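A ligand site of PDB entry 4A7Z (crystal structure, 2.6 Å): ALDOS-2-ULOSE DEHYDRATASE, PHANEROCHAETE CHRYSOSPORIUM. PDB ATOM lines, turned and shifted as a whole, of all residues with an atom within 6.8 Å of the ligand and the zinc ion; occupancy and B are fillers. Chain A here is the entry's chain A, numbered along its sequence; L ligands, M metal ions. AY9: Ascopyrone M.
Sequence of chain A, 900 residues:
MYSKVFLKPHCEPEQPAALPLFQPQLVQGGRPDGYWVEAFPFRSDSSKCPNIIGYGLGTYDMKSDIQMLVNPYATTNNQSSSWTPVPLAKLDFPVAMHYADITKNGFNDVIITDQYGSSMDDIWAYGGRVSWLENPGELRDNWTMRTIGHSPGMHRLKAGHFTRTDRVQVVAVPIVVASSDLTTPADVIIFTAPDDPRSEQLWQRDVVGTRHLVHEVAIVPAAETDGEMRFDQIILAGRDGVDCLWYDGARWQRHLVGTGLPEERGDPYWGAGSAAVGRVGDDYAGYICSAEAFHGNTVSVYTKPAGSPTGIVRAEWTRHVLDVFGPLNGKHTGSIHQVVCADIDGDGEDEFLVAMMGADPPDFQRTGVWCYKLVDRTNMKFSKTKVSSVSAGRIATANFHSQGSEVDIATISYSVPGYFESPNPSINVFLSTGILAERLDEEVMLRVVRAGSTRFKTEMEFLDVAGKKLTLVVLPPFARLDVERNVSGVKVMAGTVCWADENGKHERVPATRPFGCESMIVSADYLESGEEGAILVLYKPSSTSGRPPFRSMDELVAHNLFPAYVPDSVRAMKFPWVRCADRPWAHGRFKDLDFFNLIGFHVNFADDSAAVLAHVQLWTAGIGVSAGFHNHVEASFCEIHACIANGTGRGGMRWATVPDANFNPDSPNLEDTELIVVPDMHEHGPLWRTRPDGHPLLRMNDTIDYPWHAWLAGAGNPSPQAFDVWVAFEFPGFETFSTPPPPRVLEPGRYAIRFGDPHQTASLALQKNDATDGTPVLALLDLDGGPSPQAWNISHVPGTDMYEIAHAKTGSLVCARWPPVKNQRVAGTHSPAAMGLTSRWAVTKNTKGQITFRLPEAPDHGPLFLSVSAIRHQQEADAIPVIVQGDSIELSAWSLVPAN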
ATOM      1  N   TYR A  35      13.555   0.809  16.721  1.00  0.00           N
ATOM      2  CA  TYR A  35      12.678   0.136  15.750  1.00  0.00           C
ATOM      3  C   TYR A  35      11.455  -0.598  16.319  1.00  0.00           C
ATOM      4  O   TYR A  35      10.351  -0.429  15.817  1.00  0.00           O
ATOM      5  CB  TYR A  35      13.477  -0.901  14.966  1.00  0.00           C
ATOM      6  CG  TYR A  35      12.680  -1.451  13.826  1.00  0.00           C
ATOM      7  CD1 TYR A  35      12.452  -0.644  12.699  1.00  0.00           C
ATOM      8  CD2 TYR A  35      12.141  -2.735  13.847  1.00  0.00           C
ATOM      9  CE1 TYR A  35      11.725  -1.123  11.628  1.00  0.00           C
ATOM     10  CE2 TYR A  35      11.409  -3.216  12.739  1.00  0.00           C
ATOM     11  CZ  TYR A  35      11.213  -2.388  11.650  1.00  0.00           C
ATOM     12  OH  TYR A  35      10.518  -2.786  10.548  1.00  0.00           O
ATOM     13  N   LEU A  57      17.806  -2.294  14.630  1.00  0.00           N
ATOM     14  CA  LEU A  57      18.368  -3.308  13.751  1.00  0.00           C
ATOM     15  C   LEU A  57      19.877  -3.494  13.977  1.00  0.00           C
ATOM     16  O   LEU A  57      20.467  -4.457  13.485  1.00  0.00           O
ATOM     17  CB  LEU A  57      18.133  -2.944  12.274  1.00  0.00           C
ATOM     18  CG  LEU A  57      16.810  -2.829  11.521  1.00  0.00           C
ATOM     19  CD1 LEU A  57      17.044  -3.509  10.185  1.00  0.00           C
ATOM     20  CD2 LEU A  57      15.591  -3.442  12.191  1.00  0.00           C
ATOM     21  N   VAL A  95      14.610  -7.988  13.433  1.00  0.00           N
ATOM     22  CA  VAL A  95      13.546  -7.139  12.934  1.00  0.00           C
ATOM     23  C   VAL A  95      12.303  -7.263  13.782  1.00  0.00           C
ATOM     24  O   VAL A  95      12.129  -6.483  14.674  1.00  0.00           O
ATOM     25  CB  VAL A  95      13.208  -7.326  11.427  1.00  0.00           C
ATOM     26  CG1 VAL A  95      12.022  -6.448  11.052  1.00  0.00           C
ATOM     27  CG2 VAL A  95      14.387  -6.958  10.567  1.00  0.00           C
ATOM     28  N   TYR A 116      18.585 -10.347   9.123  1.00  0.00           N
ATOM     29  CA  TYR A 116      17.774  -9.806   8.044  1.00  0.00           C
ATOM     30  C   TYR A 116      18.631  -9.177   6.953  1.00  0.00           C
ATOM     31  O   TYR A 116      18.526  -9.513   5.769  1.00  0.00           O
ATOM     32  CB  TYR A 116      16.828  -8.770   8.623  1.00  0.00           C
ATOM     33  CG  TYR A 116      16.019  -7.975   7.634  1.00  0.00           C
ATOM     34  CD1 TYR A 116      14.895  -8.518   7.048  1.00  0.00           C
ATOM     35  CD2 TYR A 116      16.345  -6.655   7.313  1.00  0.00           C
ATOM     36  CE1 TYR A 116      14.105  -7.791   6.182  1.00  0.00           C
ATOM     37  CE2 TYR A 116      15.576  -5.910   6.434  1.00  0.00           C
ATOM     38  CZ  TYR A 116      14.438  -6.482   5.866  1.00  0.00           C
ATOM     39  OH  TYR A 116      13.618  -5.804   4.956  1.00  0.00           O
ATOM     40  N   GLY A 117      19.480  -8.246   7.376  1.00  0.00           N
ATOM     41  CA  GLY A 117      20.325  -7.457   6.493  1.00  0.00           C
ATOM     42  C   GLY A 117      20.096  -6.049   6.940  1.00  0.00           C
ATOM     43  O   GLY A 117      19.368  -5.838   7.913  1.00  0.00           O
ATOM     44  N   SER A 118      20.701  -5.076   6.251  1.00  0.00           N
ATOM     45  CA  SER A 118      20.511  -3.670   6.639  1.00  0.00           C
ATOM     46  C   SER A 118      19.343  -2.930   5.940  1.00  0.00           C
ATOM     47  O   SER A 118      18.892  -1.886   6.402  1.00  0.00           O
ATOM     48  CB  SER A 118      21.801  -2.875   6.475  1.00  0.00           C
ATOM     49  OG  SER A 118      21.909  -2.438   5.144  1.00  0.00           O
ATOM     50  N   SER A 119      18.861  -3.444   4.827  1.00  0.00           N
ATOM     51  CA  SER A 119      17.783  -2.782   4.104  1.00  0.00           C
ATOM     52  C   SER A 119      17.188  -3.711   3.035  1.00  0.00           C
ATOM     53  O   SER A 119      17.716  -4.799   2.759  1.00  0.00           O
ATOM     54  CB  SER A 119      18.303  -1.475   3.471  1.00  0.00           C
ATOM     55  OG  SER A 119      19.175  -1.720   2.372  1.00  0.00           O
ATOM     56  N   MET A 120      16.095  -3.264   2.424  1.00  0.00           N
ATOM     57  CA  MET A 120      15.484  -3.983   1.299  1.00  0.00           C
ATOM     58  C   MET A 120      16.436  -4.061   0.105  1.00  0.00           C
ATOM     59  O   MET A 120      16.199  -4.809  -0.843  1.00  0.00           O
ATOM     60  CB  MET A 120      14.121  -3.369   0.931  1.00  0.00           C
ATOM     61  CG  MET A 120      13.041  -3.825   1.891  1.00  0.00           C
ATOM     62  SD  MET A 120      11.655  -2.699   2.106  1.00  0.00           S
ATOM     63  CE  MET A 120      10.778  -2.974   0.570  1.00  0.00           C
ATOM     64  N   ASP A 121      17.516  -3.282   0.177  1.00  0.00           N
ATOM     65  CA  ASP A 121      18.548  -3.317  -0.822  1.00  0.00           C
ATOM     66  C   ASP A 121      19.743  -4.163  -0.390  1.00  0.00           C
ATOM     67  O   ASP A 121      20.628  -4.431  -1.184  1.00  0.00           O
ATOM     68  CB  ASP A 121      18.975  -1.878  -1.172  1.00  0.00           C
ATOM     69  CG  ASP A 121      17.936  -1.162  -2.014  1.00  0.00           C
ATOM     70  OD1 ASP A 121      17.510  -1.716  -3.057  1.00  0.00           O
ATOM     71  OD2 ASP A 121      17.542  -0.039  -1.643  1.00  0.00           O
ATOM     72  N   ILE A 123      19.691  -7.498   1.466  1.00  0.00           N
ATOM     73  CA  ILE A 123      19.023  -8.664   2.068  1.00  0.00           C
ATOM     74  C   ILE A 123      19.993  -9.837   2.123  1.00  0.00           C
ATOM     75  O   ILE A 123      20.629 -10.147   1.134  1.00  0.00           O
ATOM     76  CB  ILE A 123      17.768  -9.080   1.276  1.00  0.00           C
ATOM     77  CG1 ILE A 123      16.721  -7.983   1.290  1.00  0.00           C
ATOM     78  CG2 ILE A 123      17.172 -10.355   1.834  1.00  0.00           C
ATOM     79  CD1 ILE A 123      15.861  -7.954   2.535  1.00  0.00           C
ATOM     80  N   HIS A 155      10.541 -10.634   7.818  1.00  0.00           N
ATOM     81  CA  HIS A 155      10.343  -9.243   8.244  1.00  0.00           C
ATOM     82  C   HIS A 155       9.234  -8.980   9.255  1.00  0.00           C
ATOM     83  O   HIS A 155       9.227  -7.915   9.904  1.00  0.00           O
ATOM     84  CB  HIS A 155      10.190  -8.394   6.980  1.00  0.00           C
ATOM     85  CG  HIS A 155       9.695  -6.999   7.237  1.00  0.00           C
ATOM     86  ND1 HIS A 155       8.393  -6.737   7.464  1.00  0.00           N
ATOM     87  CD2 HIS A 155      10.356  -5.781   7.271  1.00  0.00           C
ATOM     88  CE1 HIS A 155       8.232  -5.410   7.637  1.00  0.00           C
ATOM     89  NE2 HIS A 155       9.438  -4.825   7.541  1.00  0.00           N
ATOM     90  N   ARG A 156       8.278  -9.903   9.402  1.00  0.00           N
ATOM     91  CA  ARG A 156       7.235  -9.799  10.409  1.00  0.00           C
ATOM     92  C   ARG A 156       6.830 -11.199  10.832  1.00  0.00           C
ATOM     93  O   ARG A 156       6.924 -12.146  10.034  1.00  0.00           O
ATOM     94  CB  ARG A 156       5.997  -9.084   9.859  1.00  0.00           C
ATOM     95  CG  ARG A 156       6.085  -7.594   9.701  1.00  0.00           C
ATOM     96  CD  ARG A 156       6.363  -6.928  11.024  1.00  0.00           C
ATOM     97  NE  ARG A 156       6.316  -5.477  10.922  1.00  0.00           N
ATOM     98  CZ  ARG A 156       7.378  -4.721  10.695  1.00  0.00           C
ATOM     99  NH1 ARG A 156       8.555  -5.285  10.476  1.00  0.00           N
ATOM    100  NH2 ARG A 156       7.271  -3.403  10.650  1.00  0.00           N
ATOM    101  N   ILE A 175       9.249  -9.576   3.522  1.00  0.00           N
ATOM    102  CA  ILE A 175       8.674  -8.439   2.847  1.00  0.00           C
ATOM    103  C   ILE A 175       9.112  -8.499   1.420  1.00  0.00           C
ATOM    104  O   ILE A 175       8.370  -8.106   0.533  1.00  0.00           O
ATOM    105  CB  ILE A 175       9.083  -7.079   3.499  1.00  0.00           C
ATOM    106  CG1 ILE A 175       8.317  -5.924   2.808  1.00  0.00           C
ATOM    107  CG2 ILE A 175      10.616  -6.880   3.531  1.00  0.00           C
ATOM    108  CD1 ILE A 175       8.442  -4.573   3.462  1.00  0.00           C
ATOM    109  N   VAL A 176      10.361  -8.949   1.204  1.00  0.00           N
ATOM    110  CA  VAL A 176      10.932  -9.150  -0.167  1.00  0.00           C
ATOM    111  C   VAL A 176      11.784 -10.430  -0.051  1.00  0.00           C
ATOM    112  O   VAL A 176      12.132 -10.853   1.095  1.00  0.00           O
ATOM    113  CB  VAL A 176      11.741  -7.913  -0.686  1.00  0.00           C
ATOM    114  CG1 VAL A 176      10.867  -6.672  -0.757  1.00  0.00           C
ATOM    115  CG2 VAL A 176      12.984  -7.604   0.167  1.00  0.00           C
ATOM    116  N   HIS A 215       3.900  -5.867   4.937  1.00  0.00           N
ATOM    117  CA  HIS A 215       4.642  -5.046   5.893  1.00  0.00           C
ATOM    118  C   HIS A 215       4.131  -5.177   7.292  1.00  0.00           C
ATOM    119  O   HIS A 215       4.788  -4.709   8.225  1.00  0.00           O
ATOM    120  CB  HIS A 215       4.667  -3.569   5.465  1.00  0.00           C
ATOM    121  CG  HIS A 215       5.478  -2.693   6.398  1.00  0.00           C
ATOM    122  ND1 HIS A 215       4.911  -1.891   7.320  1.00  0.00           N
ATOM    123  CD2 HIS A 215       6.854  -2.556   6.530  1.00  0.00           C
ATOM    124  CE1 HIS A 215       5.877  -1.270   8.012  1.00  0.00           C
ATOM    125  NE2 HIS A 215       7.065  -1.662   7.535  1.00  0.00           N
ATOM    126  N   PHE A 294       3.208   1.261   1.997  1.00  0.00           N
ATOM    127  CA  PHE A 294       4.436   1.059   2.741  1.00  0.00           C
ATOM    128  C   PHE A 294       5.070   2.396   3.169  1.00  0.00           C
ATOM    129  O   PHE A 294       5.442   3.243   2.315  1.00  0.00           O
ATOM    130  CB  PHE A 294       5.402   0.325   1.833  1.00  0.00           C
ATOM    131  CG  PHE A 294       6.789   0.277   2.356  1.00  0.00           C
ATOM    132  CD1 PHE A 294       7.101  -0.586   3.437  1.00  0.00           C
ATOM    133  CD2 PHE A 294       7.775   1.062   1.792  1.00  0.00           C
ATOM    134  CE1 PHE A 294       8.384  -0.648   3.927  1.00  0.00           C
ATOM    135  CE2 PHE A 294       9.064   1.017   2.269  1.00  0.00           C
ATOM    136  CZ  PHE A 294       9.369   0.166   3.345  1.00  0.00           C
ATOM    137  N   HIS A 295       5.191   2.561   4.494  1.00  0.00           N
ATOM    138  CA  HIS A 295       5.759   3.782   5.108  1.00  0.00           C
ATOM    139  C   HIS A 295       5.089   5.001   4.530  1.00  0.00           C
ATOM    140  O   HIS A 295       5.716   6.031   4.326  1.00  0.00           O
ATOM    141  CB  HIS A 295       7.277   3.856   4.871  1.00  0.00           C
ATOM    142  CG  HIS A 295       8.059   2.783   5.579  1.00  0.00           C
ATOM    143  ND1 HIS A 295       9.381   2.900   5.804  1.00  0.00           N
ATOM    144  CD2 HIS A 295       7.668   1.552   6.108  1.00  0.00           C
ATOM    145  CE1 HIS A 295       9.822   1.788   6.434  1.00  0.00           C
ATOM    146  NE2 HIS A 295       8.760   0.971   6.611  1.00  0.00           N
ATOM    147  N   HIS A 337       4.284   4.335  10.187  1.00  0.00           N
ATOM    148  CA  HIS A 337       4.834   2.957  10.202  1.00  0.00           C
ATOM    149  C   HIS A 337       3.900   1.868  10.670  1.00  0.00           C
ATOM    150  O   HIS A 337       4.046   0.710  10.308  1.00  0.00           O
ATOM    151  CB  HIS A 337       6.115   2.879  11.036  1.00  0.00           C
ATOM    152  CG  HIS A 337       7.001   1.685  10.675  1.00  0.00           C
ATOM    153  ND1 HIS A 337       7.423   0.784  11.592  1.00  0.00           N
ATOM    154  CD2 HIS A 337       7.546   1.295   9.468  1.00  0.00           C
ATOM    155  CE1 HIS A 337       8.206  -0.139  10.998  1.00  0.00           C
ATOM    156  NE2 HIS A 337       8.270   0.164   9.701  1.00  0.00           N
ATOM    157  N   MET A 357       6.514   8.244  12.513  1.00  0.00           N
ATOM    158  CA  MET A 357       7.967   8.136  12.515  1.00  0.00           C
ATOM    159  C   MET A 357       8.679   9.467  12.657  1.00  0.00           C
ATOM    160  O   MET A 357       9.705   9.534  13.331  1.00  0.00           O
ATOM    161  CB  MET A 357       8.429   7.510  11.217  1.00  0.00           C
ATOM    162  CG  MET A 357       7.763   6.189  10.987  1.00  0.00           C
ATOM    163  SD  MET A 357       8.387   5.537   9.475  1.00  0.00           S
ATOM    164  CE  MET A 357       7.390   6.362   8.252  1.00  0.00           C
ATOM    165  N   TYR A 414      11.562   5.876  15.794  1.00  0.00           N
ATOM    166  CA  TYR A 414      11.944   5.255  14.545  1.00  0.00           C
ATOM    167  C   TYR A 414      13.306   5.767  14.122  1.00  0.00           C
ATOM    168  O   TYR A 414      13.421   6.923  13.659  1.00  0.00           O
ATOM    169  CB  TYR A 414      10.927   5.585  13.413  1.00  0.00           C
ATOM    170  CG  TYR A 414      11.200   4.696  12.241  1.00  0.00           C
ATOM    171  CD1 TYR A 414      12.217   4.994  11.311  1.00  0.00           C
ATOM    172  CD2 TYR A 414      10.535   3.485  12.129  1.00  0.00           C
ATOM    173  CE1 TYR A 414      12.511   4.108  10.271  1.00  0.00           C
ATOM    174  CE2 TYR A 414      10.821   2.611  11.108  1.00  0.00           C
ATOM    175  CZ  TYR A 414      11.794   2.913  10.192  1.00  0.00           C
ATOM    176  OH  TYR A 414      11.974   1.978   9.214  1.00  0.00           O
ATOM    177  N   VAL A 416      16.348   4.131  11.755  1.00  0.00           N
ATOM    178  CA  VAL A 416      16.881   3.023  10.993  1.00  0.00           C
ATOM    179  C   VAL A 416      17.724   3.578   9.843  1.00  0.00           C
ATOM    180  O   VAL A 416      17.193   4.177   8.912  1.00  0.00           O
ATOM    181  CB  VAL A 416      15.754   2.078  10.473  1.00  0.00           C
ATOM    182  CG1 VAL A 416      16.336   0.940   9.634  1.00  0.00           C
ATOM    183  CG2 VAL A 416      14.954   1.503  11.635  1.00  0.00           C
ATOM    184  N   PRO A 417      19.030   3.368   9.921  1.00  0.00           N
ATOM    185  CA  PRO A 417      19.923   3.743   8.824  1.00  0.00           C
ATOM    186  C   PRO A 417      19.330   3.445   7.432  1.00  0.00           C
ATOM    187  O   PRO A 417      18.969   2.299   7.152  1.00  0.00           O
ATOM    188  CB  PRO A 417      21.176   2.892   9.099  1.00  0.00           C
ATOM    189  CG  PRO A 417      21.192   2.754  10.598  1.00  0.00           C
ATOM    190  CD  PRO A 417      19.760   2.726  11.042  1.00  0.00           C
ATOM    191  N   TYR A 419      16.520   4.965   5.969  1.00  0.00           N
ATOM    192  CA  TYR A 419      15.067   5.156   5.889  1.00  0.00           C
ATOM    193  C   TYR A 419      14.649   6.493   6.501  1.00  0.00           C
ATOM    194  O   TYR A 419      14.132   7.383   5.801  1.00  0.00           O
ATOM    195  CB  TYR A 419      14.368   4.025   6.630  1.00  0.00           C
ATOM    196  CG  TYR A 419      14.421   2.742   5.880  1.00  0.00           C
ATOM    197  CD1 TYR A 419      15.505   1.863   6.029  1.00  0.00           C
ATOM    198  CD2 TYR A 419      13.401   2.407   4.978  1.00  0.00           C
ATOM    199  CE1 TYR A 419      15.558   0.674   5.303  1.00  0.00           C
ATOM    200  CE2 TYR A 419      13.454   1.230   4.260  1.00  0.00           C
ATOM    201  CZ  TYR A 419      14.529   0.369   4.420  1.00  0.00           C
ATOM    202  OH  TYR A 419      14.573  -0.774   3.687  1.00  0.00           O
HETATM  203  C1  AY9 L   1      12.745  -0.976   8.450  1.00  0.00           C
HETATM  204  C2  AY9 L   1      11.406  -1.142   8.182  1.00  0.00           C
HETATM  205  C3  AY9 L   1      11.046  -2.032   7.189  1.00  0.00           C
HETATM  206  C4  AY9 L   1      12.008  -2.749   6.479  1.00  0.00           C
HETATM  207  C5  AY9 L   1      13.340  -2.577   6.870  1.00  0.00           C
HETATM  208  C6  AY9 L   1      14.425  -2.821   5.893  1.00  0.00           C
HETATM  209  O2  AY9 L   1      10.545  -0.473   8.755  1.00  0.00           O
HETATM  210  O3  AY9 L   1       9.734  -2.206   6.963  1.00  0.00           O
HETATM  211  O5  AY9 L   1      13.597  -1.258   7.340  1.00  0.00           O
HETATM  212  O6  AY9 L   1      13.813  -2.877   4.619  1.00  0.00           O
HETATM  213 ZN    ZN M   1       8.876  -0.647   8.027  1.00  0.00          ZN
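Ser 119 touches the ligand (CA to C6, 3.8 Å).
Phe 294 touches the ligand (CE1 to O3, 3.7 Å).
11 residues have an atom within 4 Å of the ligand: Tyr 35, Tyr 116, Ser 119, Met 120, His 155, His 215, Phe 294, His 295, His 337, Tyr 414 and Tyr 419.
The nearest printed residue that does not touch the ligand is Val 416 (4.2 Å).
O2 of the ligand sits close to OH of Tyr 414, 2.9 Å away.
O2 of the ligand lies close to OH of Tyr 35 (2.9 Å).
A ring nitrogen (NE2) of His 155 lies close to an oxygen (O3) of the ligand (2.7 Å).
The side-chain sulfur (SD) of Met 120 lies close to an oxygen (O6) of the ligand, 3.3 Å away.
The side-chain hydroxyl (OH) of Tyr 419 sits at hydrogen-bond distance from an oxygen (O6) of the ligand (2.4 Å).
N of Met 120 lies close to O6 of the ligand (3.2 Å).
The side-chain hydroxyl of Tyr 116 is in hydrogen-bond range of an oxygen (O6) of the ligand (3.0 Å).
Residues that only touch the zinc ion: Tyr 35 (3.7 Å).
Within 4 Å of the zinc ion: Tyr 35, His 215, His 295 and His 337.
The nearest printed residue that does not touch the zinc ion is Arg 156 (4.1 Å).
The guanidinium group (NH1) of Arg 156 sits close to a ring nitrogen (NE2) of His 155 (3.1 Å).
The backbone carbonyl oxygen of His 215 is in hydrogen-bond range of the guanidinium group of Arg 156, 3.2 Å away.
N of Asp 121 lies close to OG of Ser 119 (3.2 Å).
The guanidinium group (NH1) of Arg 156 sits at hydrogen-bond distance from the side-chain hydroxyl (OH) of Tyr 35 (3.2 Å).
The side-chain hydroxyl (OH) of Tyr 419 sits at hydrogen-bond distance from the backbone NH (N) of Met 120.
The zinc ion is bound by O2 of the ligand (1.8 Å), NE2 of His 337 (2.0 Å), O3 of the ligand (2.1 Å), NE2 of His 215 (2.1 Å) and NE2 of His 295 (2.2 Å).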
